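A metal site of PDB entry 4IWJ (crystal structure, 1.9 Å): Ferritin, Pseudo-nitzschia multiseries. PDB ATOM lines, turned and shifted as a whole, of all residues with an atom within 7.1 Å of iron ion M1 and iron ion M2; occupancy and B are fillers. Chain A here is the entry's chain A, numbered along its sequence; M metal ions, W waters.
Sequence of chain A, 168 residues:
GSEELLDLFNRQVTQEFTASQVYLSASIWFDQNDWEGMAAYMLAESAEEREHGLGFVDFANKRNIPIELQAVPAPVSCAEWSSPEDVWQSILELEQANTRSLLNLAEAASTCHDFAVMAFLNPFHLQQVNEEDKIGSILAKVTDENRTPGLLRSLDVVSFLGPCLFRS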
ATOM      1  N   GLN A  12      27.970   0.684 -13.035  1.00  0.00           N
ATOM      2  CA  GLN A  12      28.465   0.276 -14.416  1.00  0.00           C
ATOM      3  C   GLN A  12      28.175  -1.226 -14.592  1.00  0.00           C
ATOM      4  O   GLN A  12      27.744  -1.669 -15.648  1.00  0.00           O
ATOM      5  CB  GLN A  12      29.970   0.631 -14.629  1.00  0.00           C
ATOM      6  CG  GLN A  12      30.446   0.265 -16.084  1.00  0.00           C
ATOM      7  CD  GLN A  12      29.629   1.128 -17.077  1.00  0.00           C
ATOM      8  OE1 GLN A  12      29.185   2.212 -16.736  1.00  0.00           O
ATOM      9  NE2 GLN A  12      29.377   0.634 -18.223  1.00  0.00           N
ATOM     10  N   GLN A  15      24.606  -1.557 -15.444  1.00  0.00           N
ATOM     11  CA  GLN A  15      24.377  -1.094 -16.788  1.00  0.00           C
ATOM     12  C   GLN A  15      24.773  -2.177 -17.802  1.00  0.00           C
ATOM     13  O   GLN A  15      24.085  -2.381 -18.786  1.00  0.00           O
ATOM     14  CB  GLN A  15      25.099   0.261 -17.030  1.00  0.00           C
ATOM     15  CG  GLN A  15      24.982   0.718 -18.475  1.00  0.00           C
ATOM     16  CD  GLN A  15      23.559   1.154 -18.841  1.00  0.00           C
ATOM     17  OE1 GLN A  15      22.801   1.647 -17.973  1.00  0.00           O
ATOM     18  NE2 GLN A  15      23.173   0.998 -20.171  1.00  0.00           N
ATOM     19  N   GLU A  16      25.881  -2.860 -17.573  1.00  0.00           N
ATOM     20  CA  GLU A  16      26.317  -3.923 -18.531  1.00  0.00           C
ATOM     21  C   GLU A  16      25.309  -5.059 -18.458  1.00  0.00           C
ATOM     22  O   GLU A  16      24.898  -5.586 -19.505  1.00  0.00           O
ATOM     23  CB  GLU A  16      27.674  -4.474 -18.145  1.00  0.00           C
ATOM     24  CG  GLU A  16      28.779  -3.433 -18.108  1.00  0.00           C
ATOM     25  CD  GLU A  16      29.069  -2.880 -19.503  1.00  0.00           C
ATOM     26  OE1 GLU A  16      28.667  -3.532 -20.493  1.00  0.00           O
ATOM     27  OE2 GLU A  16      29.587  -1.742 -19.619  1.00  0.00           O
ATOM     28  N   ALA A  19      22.152  -3.991 -20.221  1.00  0.00           N
ATOM     29  CA  ALA A  19      22.347  -4.046 -21.675  1.00  0.00           C
ATOM     30  C   ALA A  19      22.250  -5.496 -22.114  1.00  0.00           C
ATOM     31  O   ALA A  19      21.613  -5.772 -23.147  1.00  0.00           O
ATOM     32  CB  ALA A  19      23.739  -3.449 -22.059  1.00  0.00           C
ATOM     33  N   TYR A  23      19.550  -6.707 -25.004  1.00  0.00           N
ATOM     34  CA  TYR A  23      19.939  -7.509 -26.197  1.00  0.00           C
ATOM     35  C   TYR A  23      19.187  -8.791 -26.234  1.00  0.00           C
ATOM     36  O   TYR A  23      18.795  -9.230 -27.314  1.00  0.00           O
ATOM     37  CB  TYR A  23      21.475  -7.773 -26.193  1.00  0.00           C
ATOM     38  CG  TYR A  23      22.256  -6.651 -26.855  1.00  0.00           C
ATOM     39  CD1 TYR A  23      23.160  -5.870 -26.114  1.00  0.00           C
ATOM     40  CD2 TYR A  23      22.169  -6.472 -28.253  1.00  0.00           C
ATOM     41  CE1 TYR A  23      23.883  -4.882 -26.711  1.00  0.00           C
ATOM     42  CE2 TYR A  23      22.871  -5.425 -28.875  1.00  0.00           C
ATOM     43  CZ  TYR A  23      23.740  -4.653 -28.097  1.00  0.00           C
ATOM     44  OH  TYR A  23      24.503  -3.687 -28.703  1.00  0.00           O
ATOM     45  N   GLU A  45      25.554 -10.508 -28.795  1.00  0.00           N
ATOM     46  CA  GLU A  45      25.803  -9.290 -28.076  1.00  0.00           C
ATOM     47  C   GLU A  45      25.370  -9.373 -26.601  1.00  0.00           C
ATOM     48  O   GLU A  45      25.987  -8.738 -25.753  1.00  0.00           O
ATOM     49  CB  GLU A  45      25.090  -8.059 -28.736  1.00  0.00           C
ATOM     50  CG  GLU A  45      25.764  -7.612 -30.007  1.00  0.00           C
ATOM     51  CD  GLU A  45      27.213  -7.251 -29.703  1.00  0.00           C
ATOM     52  OE1 GLU A  45      27.465  -6.495 -28.730  1.00  0.00           O
ATOM     53  OE2 GLU A  45      28.109  -7.781 -30.393  1.00  0.00           O
ATOM     54  N   GLU A  48      28.143 -10.941 -24.776  1.00  0.00           N
ATOM     55  CA  GLU A  48      29.321 -10.094 -24.647  1.00  0.00           C
ATOM     56  C   GLU A  48      29.124  -8.997 -23.546  1.00  0.00           C
ATOM     57  O   GLU A  48      30.105  -8.630 -22.836  1.00  0.00           O
ATOM     58  CB  GLU A  48      29.599  -9.450 -25.979  1.00  0.00           C
ATOM     59  CG  GLU A  48      30.657  -8.409 -26.003  1.00  0.00           C
ATOM     60  CD  GLU A  48      30.666  -7.716 -27.344  1.00  0.00           C
ATOM     61  OE1 GLU A  48      30.604  -8.466 -28.374  1.00  0.00           O
ATOM     62  OE2 GLU A  48      30.710  -6.454 -27.367  1.00  0.00           O
ATOM     63  N   GLU A  49      27.931  -8.433 -23.478  1.00  0.00           N
ATOM     64  CA  GLU A  49      27.683  -7.426 -22.453  1.00  0.00           C
ATOM     65  C   GLU A  49      27.780  -8.039 -21.096  1.00  0.00           C
ATOM     66  O   GLU A  49      28.242  -7.386 -20.157  1.00  0.00           O
ATOM     67  CB  GLU A  49      26.240  -6.835 -22.615  1.00  0.00           C
ATOM     68  CG  GLU A  49      26.039  -6.064 -23.908  1.00  0.00           C
ATOM     69  CD  GLU A  49      26.780  -4.746 -23.869  1.00  0.00           C
ATOM     70  OE1 GLU A  49      27.402  -4.444 -22.884  1.00  0.00           O
ATOM     71  OE2 GLU A  49      26.680  -3.948 -24.764  1.00  0.00           O
ATOM     72  N   ARG A  50      27.263  -9.296 -20.927  1.00  0.00           N
ATOM     73  CA  ARG A  50      27.425  -9.954 -19.673  1.00  0.00           C
ATOM     74  C   ARG A  50      28.953 -10.113 -19.390  1.00  0.00           C
ATOM     75  O   ARG A  50      29.414  -9.907 -18.263  1.00  0.00           O
ATOM     76  CB  ARG A  50      26.688 -11.328 -19.669  1.00  0.00           C
ATOM     77  CG  ARG A  50      26.872 -12.084 -18.330  1.00  0.00           C
ATOM     78  CD  ARG A  50      25.807 -13.220 -18.093  1.00  0.00           C
ATOM     79  NE  ARG A  50      26.043 -13.902 -16.800  1.00  0.00           N
ATOM     80  CZ  ARG A  50      26.990 -14.846 -16.750  1.00  0.00           C
ATOM     81  NH1 ARG A  50      27.672 -15.106 -17.874  1.00  0.00           N
ATOM     82  NH2 ARG A  50      27.326 -15.474 -15.644  1.00  0.00           N
ATOM     83  N   HIS A  52      31.393  -8.120 -20.333  1.00  0.00           N
ATOM     84  CA  HIS A  52      31.833  -6.822 -19.841  1.00  0.00           C
ATOM     85  C   HIS A  52      31.489  -6.663 -18.374  1.00  0.00           C
ATOM     86  O   HIS A  52      32.338  -6.206 -17.613  1.00  0.00           O
ATOM     87  CB  HIS A  52      31.172  -5.638 -20.607  1.00  0.00           C
ATOM     88  CG  HIS A  52      31.488  -5.626 -22.081  1.00  0.00           C
ATOM     89  ND1 HIS A  52      30.758  -4.904 -23.011  1.00  0.00           N
ATOM     90  CD2 HIS A  52      32.453  -6.284 -22.776  1.00  0.00           C
ATOM     91  CE1 HIS A  52      31.255  -5.124 -24.210  1.00  0.00           C
ATOM     92  NE2 HIS A  52      32.283  -5.951 -24.104  1.00  0.00           N
ATOM     93  N   GLY A  53      30.222  -6.969 -17.980  1.00  0.00           N
ATOM     94  CA  GLY A  53      29.866  -6.815 -16.565  1.00  0.00           C
ATOM     95  C   GLY A  53      30.789  -7.654 -15.700  1.00  0.00           C
ATOM     96  O   GLY A  53      31.233  -7.182 -14.606  1.00  0.00           O
ATOM     97  N   PHE A  56      34.156  -6.013 -15.176  1.00  0.00           N
ATOM     98  CA  PHE A  56      34.070  -5.000 -14.090  1.00  0.00           C
ATOM     99  C   PHE A  56      34.020  -5.590 -12.693  1.00  0.00           C
ATOM    100  O   PHE A  56      34.694  -5.057 -11.794  1.00  0.00           O
ATOM    101  CB  PHE A  56      32.874  -4.029 -14.296  1.00  0.00           C
ATOM    102  CG  PHE A  56      33.176  -2.946 -15.282  1.00  0.00           C
ATOM    103  CD1 PHE A  56      33.263  -3.263 -16.645  1.00  0.00           C
ATOM    104  CD2 PHE A  56      33.494  -1.649 -14.876  1.00  0.00           C
ATOM    105  CE1 PHE A  56      33.575  -2.308 -17.584  1.00  0.00           C
ATOM    106  CE2 PHE A  56      33.850  -0.680 -15.829  1.00  0.00           C
ATOM    107  CZ  PHE A  56      33.879  -1.012 -17.180  1.00  0.00           C
ATOM    108  N   LEU A  94      20.827   2.244 -26.514  1.00  0.00           N
ATOM    109  CA  LEU A  94      21.406   1.485 -25.368  1.00  0.00           C
ATOM    110  C   LEU A  94      22.967   1.636 -25.427  1.00  0.00           C
ATOM    111  O   LEU A  94      23.651   1.870 -24.397  1.00  0.00           O
ATOM    112  CB  LEU A  94      21.026  -0.005 -25.532  1.00  0.00           C
ATOM    113  CG  LEU A  94      21.605  -0.992 -24.519  1.00  0.00           C
ATOM    114  CD1 LEU A  94      20.758  -0.784 -23.251  1.00  0.00           C
ATOM    115  CD2 LEU A  94      21.432  -2.393 -25.126  1.00  0.00           C
ATOM    116  N   GLU A  95      23.547   1.555 -26.636  1.00  0.00           N
ATOM    117  CA  GLU A  95      24.986   1.679 -26.725  1.00  0.00           C
ATOM    118  C   GLU A  95      25.464   3.126 -26.440  1.00  0.00           C
ATOM    119  O   GLU A  95      26.511   3.302 -25.764  1.00  0.00           O
ATOM    120  CB  GLU A  95      25.501   1.148 -28.079  1.00  0.00           C
ATOM    121  CG  GLU A  95      25.284  -0.363 -28.176  1.00  0.00           C
ATOM    122  CD  GLU A  95      26.266  -1.120 -27.274  1.00  0.00           C
ATOM    123  OE1 GLU A  95      27.133  -0.495 -26.615  1.00  0.00           O
ATOM    124  OE2 GLU A  95      26.121  -2.346 -27.226  1.00  0.00           O
ATOM    125  N   ASN A  98      25.419   3.178 -22.730  1.00  0.00           N
ATOM    126  CA  ASN A  98      26.625   2.429 -22.242  1.00  0.00           C
ATOM    127  C   ASN A  98      27.849   3.390 -22.312  1.00  0.00           C
ATOM    128  O   ASN A  98      28.654   3.439 -21.379  1.00  0.00           O
ATOM    129  CB  ASN A  98      26.983   1.145 -23.059  1.00  0.00           C
ATOM    130  CG  ASN A  98      25.980  -0.061 -22.900  1.00  0.00           C
ATOM    131  OD1 ASN A  98      26.021  -1.016 -23.716  1.00  0.00           O
ATOM    132  ND2 ASN A  98      25.152  -0.059 -21.837  1.00  0.00           N
ATOM    133  N   LEU A 102      30.199   4.938 -19.159  1.00  0.00           N
ATOM    134  CA  LEU A 102      31.662   4.739 -19.099  1.00  0.00           C
ATOM    135  C   LEU A 102      32.404   6.071 -18.990  1.00  0.00           C
ATOM    136  O   LEU A 102      33.347   6.155 -18.244  1.00  0.00           O
ATOM    137  CB  LEU A 102      32.186   3.991 -20.348  1.00  0.00           C
ATOM    138  CG  LEU A 102      31.814   2.524 -20.328  1.00  0.00           C
ATOM    139  CD1 LEU A 102      32.092   1.855 -21.692  1.00  0.00           C
ATOM    140  CD2 LEU A 102      32.645   1.716 -19.280  1.00  0.00           C
ATOM    141  N   PHE A 124      37.642  -0.250 -22.980  1.00  0.00           N
ATOM    142  CA  PHE A 124      36.177  -0.156 -23.093  1.00  0.00           C
ATOM    143  C   PHE A 124      35.834   1.149 -23.810  1.00  0.00           C
ATOM    144  O   PHE A 124      34.867   1.179 -24.593  1.00  0.00           O
ATOM    145  CB  PHE A 124      35.437  -0.185 -21.739  1.00  0.00           C
ATOM    146  CG  PHE A 124      35.618  -1.508 -20.998  1.00  0.00           C
ATOM    147  CD1 PHE A 124      34.750  -2.615 -21.287  1.00  0.00           C
ATOM    148  CD2 PHE A 124      36.700  -1.663 -20.108  1.00  0.00           C
ATOM    149  CE1 PHE A 124      34.926  -3.843 -20.648  1.00  0.00           C
ATOM    150  CE2 PHE A 124      36.889  -2.901 -19.454  1.00  0.00           C
ATOM    151  CZ  PHE A 124      35.991  -3.996 -19.741  1.00  0.00           C
ATOM    152  N   GLN A 127      36.384   0.260 -27.472  1.00  0.00           N
ATOM    153  CA  GLN A 127      35.392  -0.702 -27.906  1.00  0.00           C
ATOM    154  C   GLN A 127      34.017   0.014 -28.109  1.00  0.00           C
ATOM    155  O   GLN A 127      33.299  -0.308 -29.026  1.00  0.00           O
ATOM    156  CB  GLN A 127      35.300  -1.821 -26.863  1.00  0.00           C
ATOM    157  CG  GLN A 127      34.760  -3.114 -27.447  1.00  0.00           C
ATOM    158  CD  GLN A 127      33.821  -3.841 -26.496  1.00  0.00           C
ATOM    159  OE1 GLN A 127      33.995  -3.806 -25.247  1.00  0.00           O
ATOM    160  NE2 GLN A 127      32.796  -4.525 -27.082  1.00  0.00           N
ATOM    161  N   GLN A 128      33.621   0.934 -27.262  1.00  0.00           N
ATOM    162  CA  GLN A 128      32.363   1.667 -27.487  1.00  0.00           C
ATOM    163  C   GLN A 128      32.360   2.466 -28.768  1.00  0.00           C
ATOM    164  O   GLN A 128      31.330   2.581 -29.402  1.00  0.00           O
ATOM    165  CB  GLN A 128      32.034   2.642 -26.347  1.00  0.00           C
ATOM    166  CG  GLN A 128      31.543   1.903 -25.111  1.00  0.00           C
ATOM    167  CD  GLN A 128      30.394   0.907 -25.413  1.00  0.00           C
ATOM    168  OE1 GLN A 128      30.606  -0.311 -25.390  1.00  0.00           O
ATOM    169  NE2 GLN A 128      29.198   1.412 -25.749  1.00  0.00           N
ATOM    170  N   GLU A 131      31.639  -0.066 -31.390  1.00  0.00           N
ATOM    171  CA  GLU A 131      30.282  -0.606 -31.270  1.00  0.00           C
ATOM    172  C   GLU A 131      29.237   0.427 -31.749  1.00  0.00           C
ATOM    173  O   GLU A 131      28.257   0.073 -32.430  1.00  0.00           O
ATOM    174  CB  GLU A 131      29.971  -0.980 -29.767  1.00  0.00           C
ATOM    175  CG  GLU A 131      30.599  -2.300 -29.314  1.00  0.00           C
ATOM    176  CD  GLU A 131      29.733  -3.527 -29.590  1.00  0.00           C
ATOM    177  OE1 GLU A 131      28.712  -3.450 -30.340  1.00  0.00           O
ATOM    178  OE2 GLU A 131      30.073  -4.595 -29.022  1.00  0.00           O
ATOM    179  N   ILE A 135      26.712  -0.359 -34.945  1.00  0.00           N
ATOM    180  CA  ILE A 135      25.266  -0.343 -34.802  1.00  0.00           C
ATOM    181  C   ILE A 135      24.673   0.725 -35.699  1.00  0.00           C
ATOM    182  O   ILE A 135      23.696   0.473 -36.450  1.00  0.00           O
ATOM    183  CB  ILE A 135      24.816  -0.066 -33.367  1.00  0.00           C
ATOM    184  CG1 ILE A 135      25.110  -1.285 -32.500  1.00  0.00           C
ATOM    185  CG2 ILE A 135      23.324   0.213 -33.344  1.00  0.00           C
ATOM    186  CD1 ILE A 135      24.937  -1.011 -31.042  1.00  0.00           C
HETATM  187 FE    FE M   1      29.100  -3.118 -22.591  1.00  0.00          FE
HETATM  188 FE    FE M   2      27.879  -3.474 -26.291  1.00  0.00          FE
HETATM  189  O   HOH W   1      30.645  -1.416 -22.108  1.00  0.00           O
HETATM  190  O   HOH W   2      28.806  -2.301 -24.894  1.00  0.00           O
HETATM  191  O   HOH W   3      28.378  -5.071 -27.301  1.00  0.00           O
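The side-chain amide nitrogen (ND2) of Asn 98 sits close to the side-chain amide nitrogen (NE2) of Gln 15, at 2.8 Å. The side-chain amide oxygen (OE1) of Gln 127 lies within hydrogen-bond range of a ring nitrogen (NE2) of His 52 (3.0 Å). OD1 of Asn 98 lies close to OE1 of Glu 95, 3.1 Å away. The side-chain carboxylate (OE1) of Glu 95 lies within hydrogen-bond range of the side-chain amide nitrogen (NE2) of Gln 128 (2.9 Å). The side-chain carboxylate of Glu 16 sits at hydrogen-bond distance from the side-chain amide nitrogen of Gln 12, 2.8 Å away. OE2 of Glu 49 sits close to OD1 of Asn 98, 3.2 Å away. OE2 of Glu 48 sits close to OE2 of Glu 131 (2.6 Å). OE2 of Glu 131 is in hydrogen-bond range of NE2 of Gln 127 (3.3 Å).
Glu 45 touches iron ion M2 (OE1 to FE, 3.9 Å). Glu 131 touches iron ion M2. Within 4 Å of iron ion M2: Glu 45, Glu 49, Glu 95 and Glu 131.
Iron ion M2 is bound by water W3 (2.0 Å), the side-chain carboxylate of Glu 49 (2.0 Å), water W2 (2.0 Å) and the side-chain carboxylate of Glu 95 (2.3 Å). Iron ion M2 has four donor atoms within binding distance.
Iron ion M1 is bound by the side-chain carboxylate (OE1) of Glu 49 (2.2 Å). The side-chain carboxylate (OE1) of Glu 16 is bound to iron ion M1 (2.2 Å). Iron ion M1 is bound by water W1 (2.3 Å). Water W2 binds iron ion M1, at 2.5 Å. Iron ion M1 is bound by a ring nitrogen (ND1) of His 52, at 2.5 Å. Iron ion M1 has five donor atoms within binding distance.
Residues that only touch iron ion M1: Asn 98 (3.9 Å). Within 4 Å of iron ion M1: Glu 16, Glu 49, His 52 and Asn 98. The nearest printed residue that does not touch iron ion M1 is Gln 128 (4.2 Å).
Water W1 bridges the side-chain carboxylate of Glu 16 (2.7 Å) and the side-chain amide oxygen of Gln 128 (3.5 Å). Water W3 lies within hydrogen-bond range of the side-chain carboxylate of Glu 131 (2.5 Å) and the side-chain carboxylate of Glu 48 (2.7 Å).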
